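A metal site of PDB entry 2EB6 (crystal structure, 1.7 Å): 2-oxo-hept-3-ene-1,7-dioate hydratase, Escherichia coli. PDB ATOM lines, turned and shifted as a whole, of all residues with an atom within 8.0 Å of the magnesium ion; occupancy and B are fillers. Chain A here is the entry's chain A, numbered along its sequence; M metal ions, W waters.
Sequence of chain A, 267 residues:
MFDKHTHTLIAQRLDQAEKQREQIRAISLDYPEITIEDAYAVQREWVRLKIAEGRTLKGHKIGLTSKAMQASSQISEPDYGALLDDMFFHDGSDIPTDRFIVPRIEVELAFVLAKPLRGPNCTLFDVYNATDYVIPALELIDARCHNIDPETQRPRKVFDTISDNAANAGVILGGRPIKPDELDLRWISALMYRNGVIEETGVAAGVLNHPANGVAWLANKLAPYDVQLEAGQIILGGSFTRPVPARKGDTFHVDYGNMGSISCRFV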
ATOM      1  N   LYS A  61      27.075  19.846 -21.428  1.00  0.00           N
ATOM      2  CA  LYS A  61      26.327  20.611 -22.413  1.00  0.00           C
ATOM      3  C   LYS A  61      27.182  20.857 -23.651  1.00  0.00           C
ATOM      4  O   LYS A  61      28.411  20.832 -23.579  1.00  0.00           O
ATOM      5  CB  LYS A  61      25.823  21.950 -21.834  1.00  0.00           C
ATOM      6  CG  LYS A  61      26.885  22.905 -21.272  1.00  0.00           C
ATOM      7  CD  LYS A  61      27.644  23.743 -22.337  1.00  0.00           C
ATOM      8  CE  LYS A  61      26.843  24.916 -22.882  1.00  0.00           C
ATOM      9  NZ  LYS A  61      26.634  26.024 -21.912  1.00  0.00           N
ATOM     10  N   ILE A  62      26.509  21.073 -24.770  1.00  0.00           N
ATOM     11  CA  ILE A  62      27.147  21.483 -26.018  1.00  0.00           C
ATOM     12  C   ILE A  62      26.623  22.877 -26.346  1.00  0.00           C
ATOM     13  O   ILE A  62      25.413  23.129 -26.262  1.00  0.00           O
ATOM     14  CB  ILE A  62      26.848  20.478 -27.167  1.00  0.00           C
ATOM     15  CG1 ILE A  62      27.424  19.096 -26.842  1.00  0.00           C
ATOM     16  CG2 ILE A  62      27.394  20.971 -28.504  1.00  0.00           C
ATOM     17  CD1 ILE A  62      26.368  18.075 -26.415  1.00  0.00           C
ATOM     18  N   GLY A  63      27.530  23.787 -26.677  1.00  0.00           N
ATOM     19  CA  GLY A  63      27.157  25.159 -27.006  1.00  0.00           C
ATOM     20  C   GLY A  63      27.795  25.611 -28.298  1.00  0.00           C
ATOM     21  O   GLY A  63      28.460  24.817 -28.974  1.00  0.00           O
ATOM     22  N   LEU A  64      27.579  26.876 -28.641  1.00  0.00           N
ATOM     23  CA  LEU A  64      28.100  27.463 -29.877  1.00  0.00           C
ATOM     24  C   LEU A  64      27.710  26.628 -31.087  1.00  0.00           C
ATOM     25  O   LEU A  64      28.532  26.360 -31.963  1.00  0.00           O
ATOM     26  CB  LEU A  64      29.626  27.642 -29.807  1.00  0.00           C
ATOM     27  CG  LEU A  64      30.151  28.631 -28.758  1.00  0.00           C
ATOM     28  CD1 LEU A  64      31.662  28.575 -28.680  1.00  0.00           C
ATOM     29  CD2 LEU A  64      29.673  30.041 -29.070  1.00  0.00           C
ATOM     30  N   THR A  65      26.452  26.208 -31.124  1.00  0.00           N
ATOM     31  CA  THR A  65      25.956  25.323 -32.170  1.00  0.00           C
ATOM     32  C   THR A  65      25.527  26.069 -33.443  1.00  0.00           C
ATOM     33  O   THR A  65      25.532  25.493 -34.526  1.00  0.00           O
ATOM     34  CB  THR A  65      24.801  24.420 -31.660  1.00  0.00           C
ATOM     35  OG1 THR A  65      23.760  25.223 -31.092  1.00  0.00           O
ATOM     36  CG2 THR A  65      25.300  23.433 -30.608  1.00  0.00           C
ATOM     37  N   ASP A  79      31.309  24.097 -28.725  1.00  0.00           N
ATOM     38  CA  ASP A  79      32.074  23.933 -27.494  1.00  0.00           C
ATOM     39  C   ASP A  79      31.319  23.038 -26.529  1.00  0.00           C
ATOM     40  O   ASP A  79      30.203  22.588 -26.820  1.00  0.00           O
ATOM     41  CB  ASP A  79      32.451  25.300 -26.864  1.00  0.00           C
ATOM     42  CG  ASP A  79      31.268  26.012 -26.200  1.00  0.00           C
ATOM     43  OD1 ASP A  79      30.123  25.535 -26.292  1.00  0.00           O
ATOM     44  OD2 ASP A  79      31.504  27.059 -25.561  1.00  0.00           O
ATOM     45  N   LEU A  83      28.236  19.737 -16.489  1.00  0.00           N
ATOM     46  CA  LEU A  83      27.092  20.057 -15.644  1.00  0.00           C
ATOM     47  C   LEU A  83      27.241  19.386 -14.278  1.00  0.00           C
ATOM     48  O   LEU A  83      27.449  18.172 -14.192  1.00  0.00           O
ATOM     49  CB  LEU A  83      25.783  19.618 -16.312  1.00  0.00           C
ATOM     50  CG  LEU A  83      25.444  20.264 -17.655  1.00  0.00           C
ATOM     51  CD1 LEU A  83      24.148  19.688 -18.198  1.00  0.00           C
ATOM     52  CD2 LEU A  83      25.373  21.785 -17.543  1.00  0.00           C
ATOM     53  N   ILE A 105      18.695  32.930 -20.352  1.00  0.00           N
ATOM     54  CA  ILE A 105      17.990  31.663 -20.496  1.00  0.00           C
ATOM     55  C   ILE A 105      17.998  31.173 -21.947  1.00  0.00           C
ATOM     56  O   ILE A 105      17.703  31.941 -22.862  1.00  0.00           O
ATOM     57  CB  ILE A 105      16.527  31.795 -19.995  1.00  0.00           C
ATOM     58  CG1 ILE A 105      16.496  32.034 -18.475  1.00  0.00           C
ATOM     59  CG2 ILE A 105      15.665  30.588 -20.445  1.00  0.00           C
ATOM     60  CD1 ILE A 105      16.814  30.798 -17.624  1.00  0.00           C
ATOM     61  N   GLU A 106      18.356  29.902 -22.132  1.00  0.00           N
ATOM     62  CA  GLU A 106      18.369  29.221 -23.435  1.00  0.00           C
ATOM     63  C   GLU A 106      17.348  28.074 -23.466  1.00  0.00           C
ATOM     64  O   GLU A 106      17.016  27.513 -22.429  1.00  0.00           O
ATOM     65  CB  GLU A 106      19.749  28.612 -23.704  1.00  0.00           C
ATOM     66  CG  GLU A 106      20.854  29.591 -23.886  1.00  0.00           C
ATOM     67  CD  GLU A 106      22.130  28.900 -24.296  1.00  0.00           C
ATOM     68  OE1 GLU A 106      22.504  27.876 -23.673  1.00  0.00           O
ATOM     69  OE2 GLU A 106      22.762  29.371 -25.256  1.00  0.00           O
ATOM     70  N   VAL A 107      16.895  27.722 -24.674  1.00  0.00           N
ATOM     71  CA  VAL A 107      15.858  26.704 -24.858  1.00  0.00           C
ATOM     72  C   VAL A 107      16.457  25.488 -25.558  1.00  0.00           C
ATOM     73  O   VAL A 107      16.946  25.598 -26.665  1.00  0.00           O
ATOM     74  CB  VAL A 107      14.686  27.277 -25.679  1.00  0.00           C
ATOM     75  CG1 VAL A 107      13.658  26.198 -26.008  1.00  0.00           C
ATOM     76  CG2 VAL A 107      14.046  28.443 -24.923  1.00  0.00           C
ATOM     77  N   GLU A 108      16.418  24.332 -24.886  1.00  0.00           N
ATOM     78  CA  GLU A 108      17.128  23.158 -25.385  1.00  0.00           C
ATOM     79  C   GLU A 108      16.335  21.860 -25.244  1.00  0.00           C
ATOM     80  O   GLU A 108      15.218  21.840 -24.699  1.00  0.00           O
ATOM     81  CB  GLU A 108      18.476  23.009 -24.648  1.00  0.00           C
ATOM     82  CG  GLU A 108      19.195  24.311 -24.415  1.00  0.00           C
ATOM     83  CD  GLU A 108      20.705  24.188 -24.313  1.00  0.00           C
ATOM     84  OE1 GLU A 108      21.260  23.071 -24.439  1.00  0.00           O
ATOM     85  OE2 GLU A 108      21.338  25.244 -24.137  1.00  0.00           O
ATOM     86  N   ALA A 137      14.614  21.086 -21.835  1.00  0.00           N
ATOM     87  CA  ALA A 137      15.508  21.618 -20.821  1.00  0.00           C
ATOM     88  C   ALA A 137      15.839  23.059 -21.129  1.00  0.00           C
ATOM     89  O   ALA A 137      16.119  23.412 -22.274  1.00  0.00           O
ATOM     90  CB  ALA A 137      16.793  20.794 -20.766  1.00  0.00           C
ATOM     91  N   LEU A 138      15.790  23.888 -20.088  1.00  0.00           N
ATOM     92  CA  LEU A 138      16.306  25.250 -20.186  1.00  0.00           C
ATOM     93  C   LEU A 138      17.709  25.262 -19.636  1.00  0.00           C
ATOM     94  O   LEU A 138      17.999  24.585 -18.646  1.00  0.00           O
ATOM     95  CB  LEU A 138      15.458  26.217 -19.358  1.00  0.00           C
ATOM     96  CG  LEU A 138      13.956  26.259 -19.682  1.00  0.00           C
ATOM     97  CD1 LEU A 138      13.286  27.376 -18.900  1.00  0.00           C
ATOM     98  CD2 LEU A 138      13.749  26.438 -21.196  1.00  0.00           C
ATOM     99  N   GLU A 139      18.593  26.016 -20.278  1.00  0.00           N
ATOM    100  CA  GLU A 139      19.894  26.302 -19.688  1.00  0.00           C
ATOM    101  C   GLU A 139      19.948  27.742 -19.211  1.00  0.00           C
ATOM    102  O   GLU A 139      19.524  28.653 -19.909  1.00  0.00           O
ATOM    103  CB  GLU A 139      21.067  26.011 -20.638  1.00  0.00           C
ATOM    104  CG  GLU A 139      22.404  26.065 -19.873  1.00  0.00           C
ATOM    105  CD  GLU A 139      23.631  25.716 -20.697  1.00  0.00           C
ATOM    106  OE1 GLU A 139      23.564  25.691 -21.949  1.00  0.00           O
ATOM    107  OE2 GLU A 139      24.682  25.491 -20.068  1.00  0.00           O
ATOM    108  N   LEU A 140      20.486  27.924 -18.016  1.00  0.00           N
ATOM    109  CA  LEU A 140      20.795  29.243 -17.495  1.00  0.00           C
ATOM    110  C   LEU A 140      22.297  29.397 -17.656  1.00  0.00           C
ATOM    111  O   LEU A 140      23.077  28.639 -17.076  1.00  0.00           O
ATOM    112  CB  LEU A 140      20.381  29.332 -16.023  1.00  0.00           C
ATOM    113  CG  LEU A 140      20.411  30.663 -15.267  1.00  0.00           C
ATOM    114  CD1 LEU A 140      19.656  30.485 -13.954  1.00  0.00           C
ATOM    115  CD2 LEU A 140      21.827  31.141 -14.987  1.00  0.00           C
ATOM    116  N   ILE A 141      22.699  30.350 -18.503  1.00  0.00           N
ATOM    117  CA  ILE A 141      24.117  30.608 -18.754  1.00  0.00           C
ATOM    118  C   ILE A 141      24.534  31.930 -18.095  1.00  0.00           C
ATOM    119  O   ILE A 141      23.695  32.771 -17.810  1.00  0.00           O
ATOM    120  CB  ILE A 141      24.447  30.605 -20.276  1.00  0.00           C
ATOM    121  CG1 ILE A 141      23.670  31.705 -21.021  1.00  0.00           C
ATOM    122  CG2 ILE A 141      24.197  29.217 -20.872  1.00  0.00           C
ATOM    123  CD1 ILE A 141      24.164  31.966 -22.464  1.00  0.00           C
ATOM    124  N   ALA A 166      32.286  26.888 -20.322  1.00  0.00           N
ATOM    125  CA  ALA A 166      31.344  27.078 -21.423  1.00  0.00           C
ATOM    126  C   ALA A 166      30.086  27.867 -21.019  1.00  0.00           C
ATOM    127  O   ALA A 166      28.997  27.647 -21.559  1.00  0.00           O
ATOM    128  CB  ALA A 166      30.974  25.722 -22.058  1.00  0.00           C
ATOM    129  N   ALA A 167      30.281  28.803 -20.087  1.00  0.00           N
ATOM    130  CA  ALA A 167      29.220  29.704 -19.578  1.00  0.00           C
ATOM    131  C   ALA A 167      28.165  29.015 -18.722  1.00  0.00           C
ATOM    132  O   ALA A 167      27.105  29.582 -18.466  1.00  0.00           O
ATOM    133  CB  ALA A 167      28.567  30.490 -20.730  1.00  0.00           C
ATOM    134  N   ASN A 168      28.444  27.794 -18.261  1.00  0.00           N
ATOM    135  CA  ASN A 168      27.492  27.034 -17.446  1.00  0.00           C
ATOM    136  C   ASN A 168      27.123  27.713 -16.139  1.00  0.00           C
ATOM    137  O   ASN A 168      27.956  28.371 -15.524  1.00  0.00           O
ATOM    138  CB  ASN A 168      28.018  25.628 -17.166  1.00  0.00           C
ATOM    139  CG  ASN A 168      28.143  24.788 -18.418  1.00  0.00           C
ATOM    140  OD1 ASN A 168      27.794  25.246 -19.511  1.00  0.00           O
ATOM    141  ND2 ASN A 168      28.632  23.563 -18.273  1.00  0.00           N
ATOM    142  N   GLY A 170      23.197  27.124 -14.741  1.00  0.00           N
ATOM    143  CA  GLY A 170      21.980  26.457 -14.301  1.00  0.00           C
ATOM    144  C   GLY A 170      21.335  25.598 -15.380  1.00  0.00           C
ATOM    145  O   GLY A 170      21.613  25.758 -16.568  1.00  0.00           O
ATOM    146  N   LEU A 236      22.835  18.215 -22.457  1.00  0.00           N
ATOM    147  CA  LEU A 236      22.108  19.313 -23.095  1.00  0.00           C
ATOM    148  C   LEU A 236      22.694  19.548 -24.476  1.00  0.00           C
ATOM    149  O   LEU A 236      23.874  19.870 -24.605  1.00  0.00           O
ATOM    150  CB  LEU A 236      22.153  20.582 -22.234  1.00  0.00           C
ATOM    151  CG  LEU A 236      20.968  20.810 -21.288  1.00  0.00           C
ATOM    152  CD1 LEU A 236      20.841  19.714 -20.232  1.00  0.00           C
ATOM    153  CD2 LEU A 236      21.079  22.174 -20.620  1.00  0.00           C
ATOM    154  N   GLY A 237      21.865  19.400 -25.504  1.00  0.00           N
ATOM    155  CA  GLY A 237      22.347  19.367 -26.887  1.00  0.00           C
ATOM    156  C   GLY A 237      22.668  20.694 -27.555  1.00  0.00           C
ATOM    157  O   GLY A 237      23.351  20.704 -28.585  1.00  0.00           O
ATOM    158  N   GLY A 238      22.201  21.796 -26.990  1.00  0.00           N
ATOM    159  CA  GLY A 238      22.373  23.111 -27.609  1.00  0.00           C
ATOM    160  C   GLY A 238      21.061  23.873 -27.688  1.00  0.00           C
ATOM    161  O   GLY A 238      19.987  23.280 -27.607  1.00  0.00           O
ATOM    162  N   SER A 239      21.150  25.188 -27.821  1.00  0.00           N
ATOM    163  CA  SER A 239      19.962  26.029 -27.786  1.00  0.00           C
ATOM    164  C   SER A 239      19.417  26.289 -29.165  1.00  0.00           C
ATOM    165  O   SER A 239      20.181  26.573 -30.096  1.00  0.00           O
ATOM    166  CB  SER A 239      20.260  27.366 -27.100  1.00  0.00           C
ATOM    167  OG  SER A 239      19.077  28.139 -26.968  1.00  0.00           O
ATOM    168  N   PHE A 240      18.104  26.192 -29.321  1.00  0.00           N
ATOM    169  CA  PHE A 240      17.548  26.618 -30.591  1.00  0.00           C
ATOM    170  C   PHE A 240      17.012  28.053 -30.607  1.00  0.00           C
ATOM    171  O   PHE A 240      16.403  28.483 -31.586  1.00  0.00           O
ATOM    172  CB  PHE A 240      16.655  25.559 -31.254  1.00  0.00           C
ATOM    173  CG  PHE A 240      15.663  24.860 -30.333  1.00  0.00           C
ATOM    174  CD1 PHE A 240      16.044  23.730 -29.601  1.00  0.00           C
ATOM    175  CD2 PHE A 240      14.336  25.269 -30.291  1.00  0.00           C
ATOM    176  CE1 PHE A 240      15.108  23.044 -28.811  1.00  0.00           C
ATOM    177  CE2 PHE A 240      13.414  24.616 -29.506  1.00  0.00           C
ATOM    178  CZ  PHE A 240      13.785  23.495 -28.765  1.00  0.00           C
ATOM    179  N   THR A 241      17.312  28.781 -29.539  1.00  0.00           N
ATOM    180  CA  THR A 241      17.031  30.212 -29.448  1.00  0.00           C
ATOM    181  C   THR A 241      18.249  30.982 -28.949  1.00  0.00           C
ATOM    182  O   THR A 241      19.116  30.442 -28.251  1.00  0.00           O
ATOM    183  CB  THR A 241      15.860  30.502 -28.474  1.00  0.00           C
ATOM    184  OG1 THR A 241      16.161  29.943 -27.181  1.00  0.00           O
ATOM    185  CG2 THR A 241      14.549  29.899 -28.976  1.00  0.00           C
ATOM    186  N   PRO A 243      19.963  33.442 -26.336  1.00  0.00           N
ATOM    187  CA  PRO A 243      19.717  33.568 -24.905  1.00  0.00           C
ATOM    188  C   PRO A 243      18.963  34.848 -24.569  1.00  0.00           C
ATOM    189  O   PRO A 243      19.120  35.859 -25.252  1.00  0.00           O
ATOM    190  CB  PRO A 243      21.130  33.631 -24.298  1.00  0.00           C
ATOM    191  CG  PRO A 243      22.027  33.059 -25.356  1.00  0.00           C
ATOM    192  CD  PRO A 243      21.401  33.488 -26.648  1.00  0.00           C
HETATM  193 MG    MG M   1      23.122  25.769 -23.818  1.00  0.00          MG
HETATM  194  O   HOH W   1      24.153  26.424 -25.332  1.00  0.00           O
HETATM  195  O   HOH W   2      23.772  23.906 -24.274  1.00  0.00           O
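The backbone NH (N) of Gly 238 lies within hydrogen-bond range of the side-chain carboxylate (OE1) of Glu 108, at 3.0 Å.
The backbone NH (N) of Glu 108 lies within hydrogen-bond range of the backbone carbonyl oxygen (O) of Ala 137 (2.8 Å).
The side-chain carboxylate (OE2) of Glu 139 is in salt-bridge range of the side-chain amino group (NZ) of Lys 61.
The side-chain carboxylate (OE2) of Glu 139 sits close to the side-chain amide oxygen (OD1) of Asn 168, 3.2 Å away.
The side-chain amide oxygen of Asn 168 sits at hydrogen-bond distance from the side-chain amino group of Lys 61 (2.8 Å).
The side-chain amino group (NZ) of Lys 61 is in hydrogen-bond range of the backbone carbonyl oxygen (O) of Ala 166 (2.9 Å).
Residues that only touch the magnesium ion: Lys 61 (3.9 Å).
The nearest printed residue that does not touch the magnesium ion is Ile 62 (4.3 Å).
The magnesium ion is bound by the side-chain carboxylate (OE2) of Glu 108 (1.9 Å), the side-chain carboxylate (OE1) of Glu 139 (1.9 Å), water W1 (1.9 Å), water W2 (2.0 Å) and the side-chain carboxylate (OE1) of Glu 106 (2.2 Å).
Water W2 lies within hydrogen-bond range of the side-chain carboxylate (OE1) of Glu 108 (2.7 Å) and the backbone carbonyl oxygen (O) of Ile 62 (2.7 Å).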
